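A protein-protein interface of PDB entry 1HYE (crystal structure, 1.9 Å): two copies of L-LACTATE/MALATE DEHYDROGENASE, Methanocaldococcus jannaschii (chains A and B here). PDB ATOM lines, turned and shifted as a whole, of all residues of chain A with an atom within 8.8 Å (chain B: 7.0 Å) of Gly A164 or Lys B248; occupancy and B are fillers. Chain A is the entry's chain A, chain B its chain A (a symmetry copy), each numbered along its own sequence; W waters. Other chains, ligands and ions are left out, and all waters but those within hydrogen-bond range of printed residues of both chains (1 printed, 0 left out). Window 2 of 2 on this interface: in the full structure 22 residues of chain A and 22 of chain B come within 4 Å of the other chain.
The backbone carbonyl oxygen (O) of Lys B248 sits at hydrogen-bond distance from the backbone NH (N) of His A166 (3.0 Å).
A ring nitrogen (NE2) of His A166 sits at hydrogen-bond distance from the guanidinium group (NH1) of Arg B249.
OD2 of Asp A168 is in salt-bridge range of NH2 of Arg B249, at 3.4 Å.
The side-chain carboxylate (OE2) of Glu A169 sits at hydrogen-bond distance from the backbone NH (N) of Leu B250 (2.7 Å).
The backbone NH (N) of Asp A168 is in hydrogen-bond range of a ring nitrogen (ND1) of His A166.
The backbone carbonyl oxygen of Glu A169 is in hydrogen-bond range of the backbone NH of Gly A192, 2.7 Å away.
The backbone NH of Glu B247 sits at hydrogen-bond distance from the backbone carbonyl oxygen of Cys B242, at 3.0 Å.
The side-chain carboxylate (OE2) of Glu B247 lies within salt-bridge range of the guanidinium group (NE) of Arg B249 (2.8 Å).
NZ of Lys B248 is in salt-bridge range of OE2 of Glu B281 (2.6 Å).
The backbone carbonyl oxygen (O) of Arg B249 lies within hydrogen-bond range of the backbone NH (N) of Ile B275.
Among the printed residues, pairs that only touch across the chains: His A166 with Glu B247, Glu A169 with Arg B249, Val A165 with Lys B248, Gly A164 with Lys B248 and Ile A191 with Leu B250.
Gly A164 touches just one residue of chain B: Lys B248.
Printed residues of chain B within 4 Å of Val A165: Lys B248 (3.5 Å).
Of the printed residues of chain B, Glu A169 touches Arg B249 and Leu B250.
Asn B245 touches none of the printed residues of chain A.
Of the printed residues of chain A, Glu B247 touches His A166.
Lys B248 touches just these residues of chain A: Gly A164, Val A165 and His A166.
The nearest residue of chain A that does not touch Lys B248 is Glu A169 (4.6 Å).
The nearest printed residue of chain A that does not touch Leu B250 is Gly A192 (4.2 Å).
Of the 16 printed residues of chain B, 4 touch a printed residue of chain A.
Hydrophobic or aromatic side chains of chain A that line the printed part of chain B: Val A165, His A166 and Ile A191.
No position is printed for both chains.
Water W1 bridges NH2 of Arg B249 (2.9 Å) and OE2 of Glu A169 (2.9 Å).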
ATOM      1  N   VAL A 157       4.242  -1.053 -22.293  1.00  0.00           N
ATOM      2  CA  VAL A 157       3.704   0.241 -21.893  1.00  0.00           C
ATOM      3  C   VAL A 157       2.290   0.114 -21.307  1.00  0.00           C
ATOM      4  O   VAL A 157       1.956   0.787 -20.322  1.00  0.00           O
ATOM      5  CB  VAL A 157       3.662   1.221 -23.099  1.00  0.00           C
ATOM      6  CG1 VAL A 157       2.947   2.509 -22.709  1.00  0.00           C
ATOM      7  CG2 VAL A 157       5.079   1.541 -23.556  1.00  0.00           C
ATOM      8  N   ALA A 158       1.472  -0.738 -21.913  1.00  0.00           N
ATOM      9  CA  ALA A 158       0.101  -0.932 -21.441  1.00  0.00           C
ATOM     10  C   ALA A 158       0.064  -1.538 -20.047  1.00  0.00           C
ATOM     11  O   ALA A 158      -0.722  -1.111 -19.196  1.00  0.00           O
ATOM     12  CB  ALA A 158      -0.681  -1.825 -22.423  1.00  0.00           C
ATOM     13  N   ILE A 159       0.916  -2.531 -19.800  1.00  0.00           N
ATOM     14  CA  ILE A 159       0.964  -3.184 -18.501  1.00  0.00           C
ATOM     15  C   ILE A 159       1.496  -2.252 -17.414  1.00  0.00           C
ATOM     16  O   ILE A 159       0.955  -2.203 -16.308  1.00  0.00           O
ATOM     17  CB  ILE A 159       1.823  -4.457 -18.561  1.00  0.00           C
ATOM     18  CG1 ILE A 159       1.185  -5.447 -19.540  1.00  0.00           C
ATOM     19  CG2 ILE A 159       1.960  -5.067 -17.161  1.00  0.00           C
ATOM     20  CD1 ILE A 159       1.986  -6.700 -19.778  1.00  0.00           C
ATOM     21  N   ALA A 160       2.547  -1.504 -17.736  1.00  0.00           N
ATOM     22  CA  ALA A 160       3.129  -0.569 -16.775  1.00  0.00           C
ATOM     23  C   ALA A 160       2.072   0.462 -16.371  1.00  0.00           C
ATOM     24  O   ALA A 160       1.969   0.840 -15.203  1.00  0.00           O
ATOM     25  CB  ALA A 160       4.344   0.132 -17.388  1.00  0.00           C
ATOM     26  N   LYS A 161       1.288   0.906 -17.347  1.00  0.00           N
ATOM     27  CA  LYS A 161       0.239   1.889 -17.110  1.00  0.00           C
ATOM     28  C   LYS A 161      -0.852   1.329 -16.202  1.00  0.00           C
ATOM     29  O   LYS A 161      -1.355   2.027 -15.324  1.00  0.00           O
ATOM     30  CB  LYS A 161      -0.379   2.326 -18.441  1.00  0.00           C
ATOM     31  CG  LYS A 161      -1.446   3.405 -18.311  1.00  0.00           C
ATOM     32  CD  LYS A 161      -0.887   4.672 -17.677  1.00  0.00           C
ATOM     33  CE  LYS A 161       0.211   5.290 -18.541  1.00  0.00           C
ATOM     34  NZ  LYS A 161      -0.249   5.554 -19.941  1.00  0.00           N
ATOM     35  N   PHE A 162      -1.204   0.063 -16.409  1.00  0.00           N
ATOM     36  CA  PHE A 162      -2.246  -0.569 -15.609  1.00  0.00           C
ATOM     37  C   PHE A 162      -1.842  -0.778 -14.153  1.00  0.00           C
ATOM     38  O   PHE A 162      -2.652  -0.597 -13.244  1.00  0.00           O
ATOM     39  CB  PHE A 162      -2.643  -1.918 -16.214  1.00  0.00           C
ATOM     40  CG  PHE A 162      -3.847  -2.538 -15.555  1.00  0.00           C
ATOM     41  CD1 PHE A 162      -5.124  -2.036 -15.796  1.00  0.00           C
ATOM     42  CD2 PHE A 162      -3.701  -3.594 -14.665  1.00  0.00           C
ATOM     43  CE1 PHE A 162      -6.239  -2.580 -15.156  1.00  0.00           C
ATOM     44  CE2 PHE A 162      -4.805  -4.142 -14.018  1.00  0.00           C
ATOM     45  CZ  PHE A 162      -6.077  -3.634 -14.266  1.00  0.00           C
ATOM     46  N   PHE A 163      -0.591  -1.177 -13.925  1.00  0.00           N
ATOM     47  CA  PHE A 163      -0.125  -1.409 -12.564  1.00  0.00           C
ATOM     48  C   PHE A 163       0.370  -0.150 -11.875  1.00  0.00           C
ATOM     49  O   PHE A 163       0.583  -0.150 -10.662  1.00  0.00           O
ATOM     50  CB  PHE A 163       0.969  -2.478 -12.548  1.00  0.00           C
ATOM     51  CG  PHE A 163       0.450  -3.880 -12.695  1.00  0.00           C
ATOM     52  CD1 PHE A 163      -0.004  -4.346 -13.926  1.00  0.00           C
ATOM     53  CD2 PHE A 163       0.368  -4.719 -11.590  1.00  0.00           C
ATOM     54  CE1 PHE A 163      -0.517  -5.634 -14.056  1.00  0.00           C
ATOM     55  CE2 PHE A 163      -0.147  -6.011 -11.711  1.00  0.00           C
ATOM     56  CZ  PHE A 163      -0.592  -6.466 -12.943  1.00  0.00           C
ATOM     57  N   GLY A 164       0.552   0.915 -12.640  1.00  0.00           N
ATOM     58  CA  GLY A 164       1.029   2.169 -12.076  1.00  0.00           C
ATOM     59  C   GLY A 164       2.474   2.106 -11.612  1.00  0.00           C
ATOM     60  O   GLY A 164       2.824   2.654 -10.568  1.00  0.00           O
ATOM     61  N   VAL A 165       3.320   1.430 -12.390  1.00  0.00           N
ATOM     62  CA  VAL A 165       4.735   1.312 -12.045  1.00  0.00           C
ATOM     63  C   VAL A 165       5.589   1.866 -13.170  1.00  0.00           C
ATOM     64  O   VAL A 165       5.121   2.012 -14.299  1.00  0.00           O
ATOM     65  CB  VAL A 165       5.152  -0.166 -11.804  1.00  0.00           C
ATOM     66  CG1 VAL A 165       4.510  -0.691 -10.539  1.00  0.00           C
ATOM     67  CG2 VAL A 165       4.749  -1.025 -13.005  1.00  0.00           C
ATOM     68  N   HIS A 166       6.844   2.174 -12.870  1.00  0.00           N
ATOM     69  CA  HIS A 166       7.748   2.708 -13.872  1.00  0.00           C
ATOM     70  C   HIS A 166       7.910   1.681 -15.000  1.00  0.00           C
ATOM     71  O   HIS A 166       7.956   0.478 -14.747  1.00  0.00           O
ATOM     72  CB  HIS A 166       9.105   3.016 -13.244  1.00  0.00           C
ATOM     73  CG  HIS A 166      10.004   3.832 -14.121  1.00  0.00           C
ATOM     74  ND1 HIS A 166      10.600   3.330 -15.255  1.00  0.00           N
ATOM     75  CD2 HIS A 166      10.389   5.130 -14.036  1.00  0.00           C
ATOM     76  CE1 HIS A 166      11.313   4.271 -15.832  1.00  0.00           C
ATOM     77  NE2 HIS A 166      11.205   5.382 -15.113  1.00  0.00           N
ATOM     78  N   ILE A 167       7.988   2.173 -16.236  1.00  0.00           N
ATOM     79  CA  ILE A 167       8.131   1.318 -17.413  1.00  0.00           C
ATOM     80  C   ILE A 167       9.286   0.323 -17.275  1.00  0.00           C
ATOM     81  O   ILE A 167       9.179  -0.824 -17.713  1.00  0.00           O
ATOM     82  CB  ILE A 167       8.346   2.177 -18.686  1.00  0.00           C
ATOM     83  CG1 ILE A 167       8.232   1.314 -19.940  1.00  0.00           C
ATOM     84  CG2 ILE A 167       9.713   2.836 -18.656  1.00  0.00           C
ATOM     85  CD1 ILE A 167       6.824   0.826 -20.218  1.00  0.00           C
ATOM     86  N   ASP A 168      10.387   0.758 -16.664  1.00  0.00           N
ATOM     87  CA  ASP A 168      11.575  -0.081 -16.485  1.00  0.00           C
ATOM     88  C   ASP A 168      11.331  -1.355 -15.687  1.00  0.00           C
ATOM     89  O   ASP A 168      12.052  -2.342 -15.847  1.00  0.00           O
ATOM     90  CB  ASP A 168      12.687   0.720 -15.800  1.00  0.00           C
ATOM     91  CG  ASP A 168      13.357   1.714 -16.727  1.00  0.00           C
ATOM     92  OD1 ASP A 168      12.859   1.932 -17.850  1.00  0.00           O
ATOM     93  OD2 ASP A 168      14.391   2.294 -16.316  1.00  0.00           O
ATOM     94  N   GLU A 169      10.321  -1.340 -14.821  1.00  0.00           N
ATOM     95  CA  GLU A 169      10.006  -2.490 -13.983  1.00  0.00           C
ATOM     96  C   GLU A 169       9.238  -3.597 -14.705  1.00  0.00           C
ATOM     97  O   GLU A 169       9.058  -4.687 -14.162  1.00  0.00           O
ATOM     98  CB  GLU A 169       9.205  -2.030 -12.762  1.00  0.00           C
ATOM     99  CG  GLU A 169       9.974  -1.047 -11.872  1.00  0.00           C
ATOM    100  CD  GLU A 169      11.061  -1.713 -11.049  1.00  0.00           C
ATOM    101  OE1 GLU A 169      11.501  -2.830 -11.413  1.00  0.00           O
ATOM    102  OE2 GLU A 169      11.492  -1.118 -10.043  1.00  0.00           O
ATOM    103  N   VAL A 170       8.783  -3.315 -15.924  1.00  0.00           N
ATOM    104  CA  VAL A 170       8.025  -4.302 -16.678  1.00  0.00           C
ATOM    105  C   VAL A 170       8.811  -4.919 -17.828  1.00  0.00           C
ATOM    106  O   VAL A 170       9.416  -4.215 -18.643  1.00  0.00           O
ATOM    107  CB  VAL A 170       6.723  -3.691 -17.262  1.00  0.00           C
ATOM    108  CG1 VAL A 170       5.934  -4.754 -18.009  1.00  0.00           C
ATOM    109  CG2 VAL A 170       5.881  -3.091 -16.144  1.00  0.00           C
ATOM    110  N   ILE A 191       7.064  -8.093 -13.174  1.00  0.00           N
ATOM    111  CA  ILE A 191       6.934  -6.717 -12.697  1.00  0.00           C
ATOM    112  C   ILE A 191       7.961  -6.643 -11.570  1.00  0.00           C
ATOM    113  O   ILE A 191       7.797  -7.287 -10.528  1.00  0.00           O
ATOM    114  CB  ILE A 191       5.536  -6.442 -12.104  1.00  0.00           C
ATOM    115  CG1 ILE A 191       4.444  -6.899 -13.078  1.00  0.00           C
ATOM    116  CG2 ILE A 191       5.391  -4.946 -11.795  1.00  0.00           C
ATOM    117  CD1 ILE A 191       4.396  -6.132 -14.368  1.00  0.00           C
ATOM    118  N   GLY A 192       9.034  -5.883 -11.772  1.00  0.00           N
ATOM    119  CA  GLY A 192      10.065  -5.806 -10.756  1.00  0.00           C
ATOM    120  C   GLY A 192      10.698  -7.179 -10.552  1.00  0.00           C
ATOM    121  O   GLY A 192      11.248  -7.473  -9.493  1.00  0.00           O
ATOM    122  N   ARG A 201      -3.937  -7.723  -8.615  1.00  0.00           N
ATOM    123  CA  ARG A 201      -4.434  -6.861  -9.676  1.00  0.00           C
ATOM    124  C   ARG A 201      -4.431  -7.554 -11.038  1.00  0.00           C
ATOM    125  O   ARG A 201      -5.161  -7.157 -11.947  1.00  0.00           O
ATOM    126  CB  ARG A 201      -3.602  -5.575  -9.730  1.00  0.00           C
ATOM    127  CG  ARG A 201      -4.135  -4.527 -10.693  1.00  0.00           C
ATOM    128  CD  ARG A 201      -3.536  -3.155 -10.406  1.00  0.00           C
ATOM    129  NE  ARG A 201      -4.121  -2.105 -11.241  1.00  0.00           N
ATOM    130  CZ  ARG A 201      -5.407  -1.769 -11.240  1.00  0.00           C
ATOM    131  NH1 ARG A 201      -5.845  -0.801 -12.036  1.00  0.00           N
ATOM    132  NH2 ARG A 201      -6.264  -2.401 -10.444  1.00  0.00           N
ATOM    133  N   CYS B 242      14.218   8.769  -7.454  1.00  0.00           N
ATOM    134  CA  CYS B 242      12.964   8.039  -7.505  1.00  0.00           C
ATOM    135  C   CYS B 242      11.888   8.816  -6.751  1.00  0.00           C
ATOM    136  O   CYS B 242      10.714   8.817  -7.129  1.00  0.00           O
ATOM    137  CB  CYS B 242      13.160   6.658  -6.884  1.00  0.00           C
ATOM    138  SG  CYS B 242      11.840   5.509  -7.240  1.00  0.00           S
ATOM    139  N   ILE B 243      12.296   9.491  -5.681  1.00  0.00           N
ATOM    140  CA  ILE B 243      11.370  10.280  -4.877  1.00  0.00           C
ATOM    141  C   ILE B 243      10.985  11.616  -5.513  1.00  0.00           C
ATOM    142  O   ILE B 243       9.799  11.909  -5.670  1.00  0.00           O
ATOM    143  CB  ILE B 243      11.957  10.561  -3.474  1.00  0.00           C
ATOM    144  CG1 ILE B 243      12.104   9.244  -2.707  1.00  0.00           C
ATOM    145  CG2 ILE B 243      11.057  11.528  -2.715  1.00  0.00           C
ATOM    146  CD1 ILE B 243      12.742   9.394  -1.334  1.00  0.00           C
ATOM    147  N   ASN B 245      11.231  12.557  -8.536  1.00  0.00           N
ATOM    148  CA  ASN B 245      10.601  12.345  -9.837  1.00  0.00           C
ATOM    149  C   ASN B 245       9.367  11.452  -9.780  1.00  0.00           C
ATOM    150  O   ASN B 245       8.772  11.142 -10.815  1.00  0.00           O
ATOM    151  CB  ASN B 245      11.616  11.760 -10.816  1.00  0.00           C
ATOM    152  CG  ASN B 245      12.588  12.800 -11.336  1.00  0.00           C
ATOM    153  OD1 ASN B 245      13.640  12.468 -11.872  1.00  0.00           O
ATOM    154  ND2 ASN B 245      12.227  14.073 -11.189  1.00  0.00           N
ATOM    155  N   ASN B 246       8.998  11.029  -8.575  1.00  0.00           N
ATOM    156  CA  ASN B 246       7.813  10.197  -8.367  1.00  0.00           C
ATOM    157  C   ASN B 246       7.810   9.055  -9.392  1.00  0.00           C
ATOM    158  O   ASN B 246       6.811   8.824 -10.076  1.00  0.00           O
ATOM    159  CB  ASN B 246       6.572  11.078  -8.549  1.00  0.00           C
ATOM    160  CG  ASN B 246       5.316  10.449  -8.001  1.00  0.00           C
ATOM    161  OD1 ASN B 246       4.210  10.783  -8.432  1.00  0.00           O
ATOM    162  ND2 ASN B 246       5.467   9.552  -7.035  1.00  0.00           N
ATOM    163  N   GLU B 247       8.926   8.338  -9.479  1.00  0.00           N
ATOM    164  CA  GLU B 247       9.090   7.261 -10.457  1.00  0.00           C
ATOM    165  C   GLU B 247       8.285   5.970 -10.304  1.00  0.00           C
ATOM    166  O   GLU B 247       8.030   5.288 -11.297  1.00  0.00           O
ATOM    167  CB  GLU B 247      10.581   6.947 -10.599  1.00  0.00           C
ATOM    168  CG  GLU B 247      11.378   8.146 -11.117  1.00  0.00           C
ATOM    169  CD  GLU B 247      12.865   7.880 -11.246  1.00  0.00           C
ATOM    170  OE1 GLU B 247      13.563   8.722 -11.854  1.00  0.00           O
ATOM    171  OE2 GLU B 247      13.343   6.844 -10.738  1.00  0.00           O
ATOM    172  N   LYS B 248       7.895   5.623  -9.084  1.00  0.00           N
ATOM    173  CA  LYS B 248       7.121   4.410  -8.843  1.00  0.00           C
ATOM    174  C   LYS B 248       7.884   3.127  -9.202  1.00  0.00           C
ATOM    175  O   LYS B 248       7.365   2.261  -9.915  1.00  0.00           O
ATOM    176  CB  LYS B 248       5.809   4.438  -9.637  1.00  0.00           C
ATOM    177  CG  LYS B 248       4.969   5.703  -9.481  1.00  0.00           C
ATOM    178  CD  LYS B 248       4.505   5.942  -8.057  1.00  0.00           C
ATOM    179  CE  LYS B 248       3.486   7.083  -8.023  1.00  0.00           C
ATOM    180  NZ  LYS B 248       3.217   7.585  -6.647  1.00  0.00           N
ATOM    181  N   ARG B 249       9.121   3.013  -8.722  1.00  0.00           N
ATOM    182  CA  ARG B 249       9.913   1.815  -8.969  1.00  0.00           C
ATOM    183  C   ARG B 249       9.683   0.893  -7.780  1.00  0.00           C
ATOM    184  O   ARG B 249       9.257   1.346  -6.715  1.00  0.00           O
ATOM    185  CB  ARG B 249      11.404   2.142  -9.071  1.00  0.00           C
ATOM    186  CG  ARG B 249      11.785   2.934 -10.311  1.00  0.00           C
ATOM    187  CD  ARG B 249      13.262   3.232 -10.306  1.00  0.00           C
ATOM    188  NE  ARG B 249      13.636   4.159 -11.370  1.00  0.00           N
ATOM    189  CZ  ARG B 249      13.911   3.799 -12.616  1.00  0.00           C
ATOM    190  NH1 ARG B 249      14.240   4.724 -13.515  1.00  0.00           N
ATOM    191  NH2 ARG B 249      13.873   2.522 -12.965  1.00  0.00           N
ATOM    192  N   LEU B 250       9.966  -0.387  -7.966  1.00  0.00           N
ATOM    193  CA  LEU B 250       9.790  -1.380  -6.909  1.00  0.00           C
ATOM    194  C   LEU B 250      11.170  -1.754  -6.388  1.00  0.00           C
ATOM    195  O   LEU B 250      11.690  -2.832  -6.679  1.00  0.00           O
ATOM    196  CB  LEU B 250       9.087  -2.621  -7.464  1.00  0.00           C
ATOM    197  CG  LEU B 250       7.698  -2.396  -8.072  1.00  0.00           C
ATOM    198  CD1 LEU B 250       7.134  -3.730  -8.525  1.00  0.00           C
ATOM    199  CD2 LEU B 250       6.764  -1.744  -7.050  1.00  0.00           C
ATOM    200  N   LEU B 251      11.765  -0.849  -5.614  1.00  0.00           N
ATOM    201  CA  LEU B 251      13.097  -1.093  -5.084  1.00  0.00           C
ATOM    202  C   LEU B 251      13.010  -1.961  -3.841  1.00  0.00           C
ATOM    203  O   LEU B 251      11.919  -2.337  -3.398  1.00  0.00           O
ATOM    204  CB  LEU B 251      13.783   0.241  -4.758  1.00  0.00           C
ATOM    205  CG  LEU B 251      13.761   1.293  -5.877  1.00  0.00           C
ATOM    206  CD1 LEU B 251      14.464   2.571  -5.398  1.00  0.00           C
ATOM    207  CD2 LEU B 251      14.451   0.740  -7.126  1.00  0.00           C
ATOM    208  N   VAL B 273       9.333  -2.526  -2.025  1.00  0.00           N
ATOM    209  CA  VAL B 273       8.422  -1.420  -1.755  1.00  0.00           C
ATOM    210  C   VAL B 273       8.231  -0.596  -3.022  1.00  0.00           C
ATOM    211  O   VAL B 273       9.086  -0.613  -3.906  1.00  0.00           O
ATOM    212  CB  VAL B 273       8.990  -0.485  -0.657  1.00  0.00           C
ATOM    213  CG1 VAL B 273       9.173  -1.243   0.643  1.00  0.00           C
ATOM    214  CG2 VAL B 273      10.315   0.098  -1.115  1.00  0.00           C
ATOM    215  N   LYS B 274       7.103   0.096  -3.127  1.00  0.00           N
ATOM    216  CA  LYS B 274       6.880   0.965  -4.270  1.00  0.00           C
ATOM    217  C   LYS B 274       7.272   2.329  -3.727  1.00  0.00           C
ATOM    218  O   LYS B 274       6.729   2.770  -2.713  1.00  0.00           O
ATOM    219  CB  LYS B 274       5.408   0.974  -4.707  1.00  0.00           C
ATOM    220  CG  LYS B 274       5.147   1.894  -5.904  1.00  0.00           C
ATOM    221  CD  LYS B 274       3.706   1.818  -6.411  1.00  0.00           C
ATOM    222  CE  LYS B 274       2.724   2.370  -5.373  1.00  0.00           C
ATOM    223  NZ  LYS B 274       1.300   2.255  -5.827  1.00  0.00           N
ATOM    224  N   ILE B 275       8.233   2.984  -4.374  1.00  0.00           N
ATOM    225  CA  ILE B 275       8.720   4.283  -3.920  1.00  0.00           C
ATOM    226  C   ILE B 275       8.252   5.410  -4.823  1.00  0.00           C
ATOM    227  O   ILE B 275       8.250   5.267  -6.047  1.00  0.00           O
ATOM    228  CB  ILE B 275      10.276   4.334  -3.873  1.00  0.00           C
ATOM    229  CG1 ILE B 275      10.833   3.112  -3.147  1.00  0.00           C
ATOM    230  CG2 ILE B 275      10.743   5.602  -3.154  1.00  0.00           C
ATOM    231  CD1 ILE B 275      10.846   1.848  -3.985  1.00  0.00           C
ATOM    232  N   GLY B 276       7.882   6.530  -4.212  1.00  0.00           N
ATOM    233  CA  GLY B 276       7.424   7.686  -4.956  1.00  0.00           C
ATOM    234  C   GLY B 276       7.641   8.968  -4.164  1.00  0.00           C
ATOM    235  O   GLY B 276       8.370   8.979  -3.169  1.00  0.00           O
ATOM    236  N   ARG B 277       6.994  10.049  -4.593  1.00  0.00           N
ATOM    237  CA  ARG B 277       7.137  11.332  -3.919  1.00  0.00           C
ATOM    238  C   ARG B 277       6.716  11.269  -2.456  1.00  0.00           C
ATOM    239  O   ARG B 277       7.127  12.100  -1.653  1.00  0.00           O
ATOM    240  CB  ARG B 277       6.310  12.406  -4.632  1.00  0.00           C
ATOM    241  CG  ARG B 277       4.832  12.081  -4.736  1.00  0.00           C
ATOM    242  CD  ARG B 277       4.008  13.354  -4.840  1.00  0.00           C
ATOM    243  NE  ARG B 277       4.484  14.232  -5.902  1.00  0.00           N
ATOM    244  CZ  ARG B 277       3.978  15.432  -6.163  1.00  0.00           C
ATOM    245  NH1 ARG B 277       4.475  16.165  -7.151  1.00  0.00           N
ATOM    246  NH2 ARG B 277       2.974  15.903  -5.431  1.00  0.00           N
ATOM    247  N   ASP B 278       5.897  10.286  -2.108  1.00  0.00           N
ATOM    248  CA  ASP B 278       5.440  10.149  -0.729  1.00  0.00           C
ATOM    249  C   ASP B 278       6.242   9.108   0.049  1.00  0.00           C
ATOM    250  O   ASP B 278       5.788   8.603   1.075  1.00  0.00           O
ATOM    251  CB  ASP B 278       3.952   9.786  -0.713  1.00  0.00           C
ATOM    252  CG  ASP B 278       3.064  10.954  -1.111  1.00  0.00           C
ATOM    253  OD1 ASP B 278       1.880  10.722  -1.431  1.00  0.00           O
ATOM    254  OD2 ASP B 278       3.549  12.104  -1.097  1.00  0.00           O
ATOM    255  N   GLU B 281       5.344   4.209  -0.481  1.00  0.00           N
ATOM    256  CA  GLU B 281       3.913   4.251  -0.725  1.00  0.00           C
ATOM    257  C   GLU B 281       3.224   2.918  -0.465  1.00  0.00           C
ATOM    258  O   GLU B 281       2.006   2.862  -0.345  1.00  0.00           O
ATOM    259  CB  GLU B 281       3.666   4.764  -2.146  1.00  0.00           C
ATOM    260  CG  GLU B 281       4.257   6.160  -2.320  1.00  0.00           C
ATOM    261  CD  GLU B 281       4.043   6.754  -3.692  1.00  0.00           C
ATOM    262  OE1 GLU B 281       4.430   7.931  -3.876  1.00  0.00           O
ATOM    263  OE2 GLU B 281       3.502   6.057  -4.576  1.00  0.00           O
HETATM  264  O   HOH W   1      13.745   0.057 -11.491  1.00  0.00           O
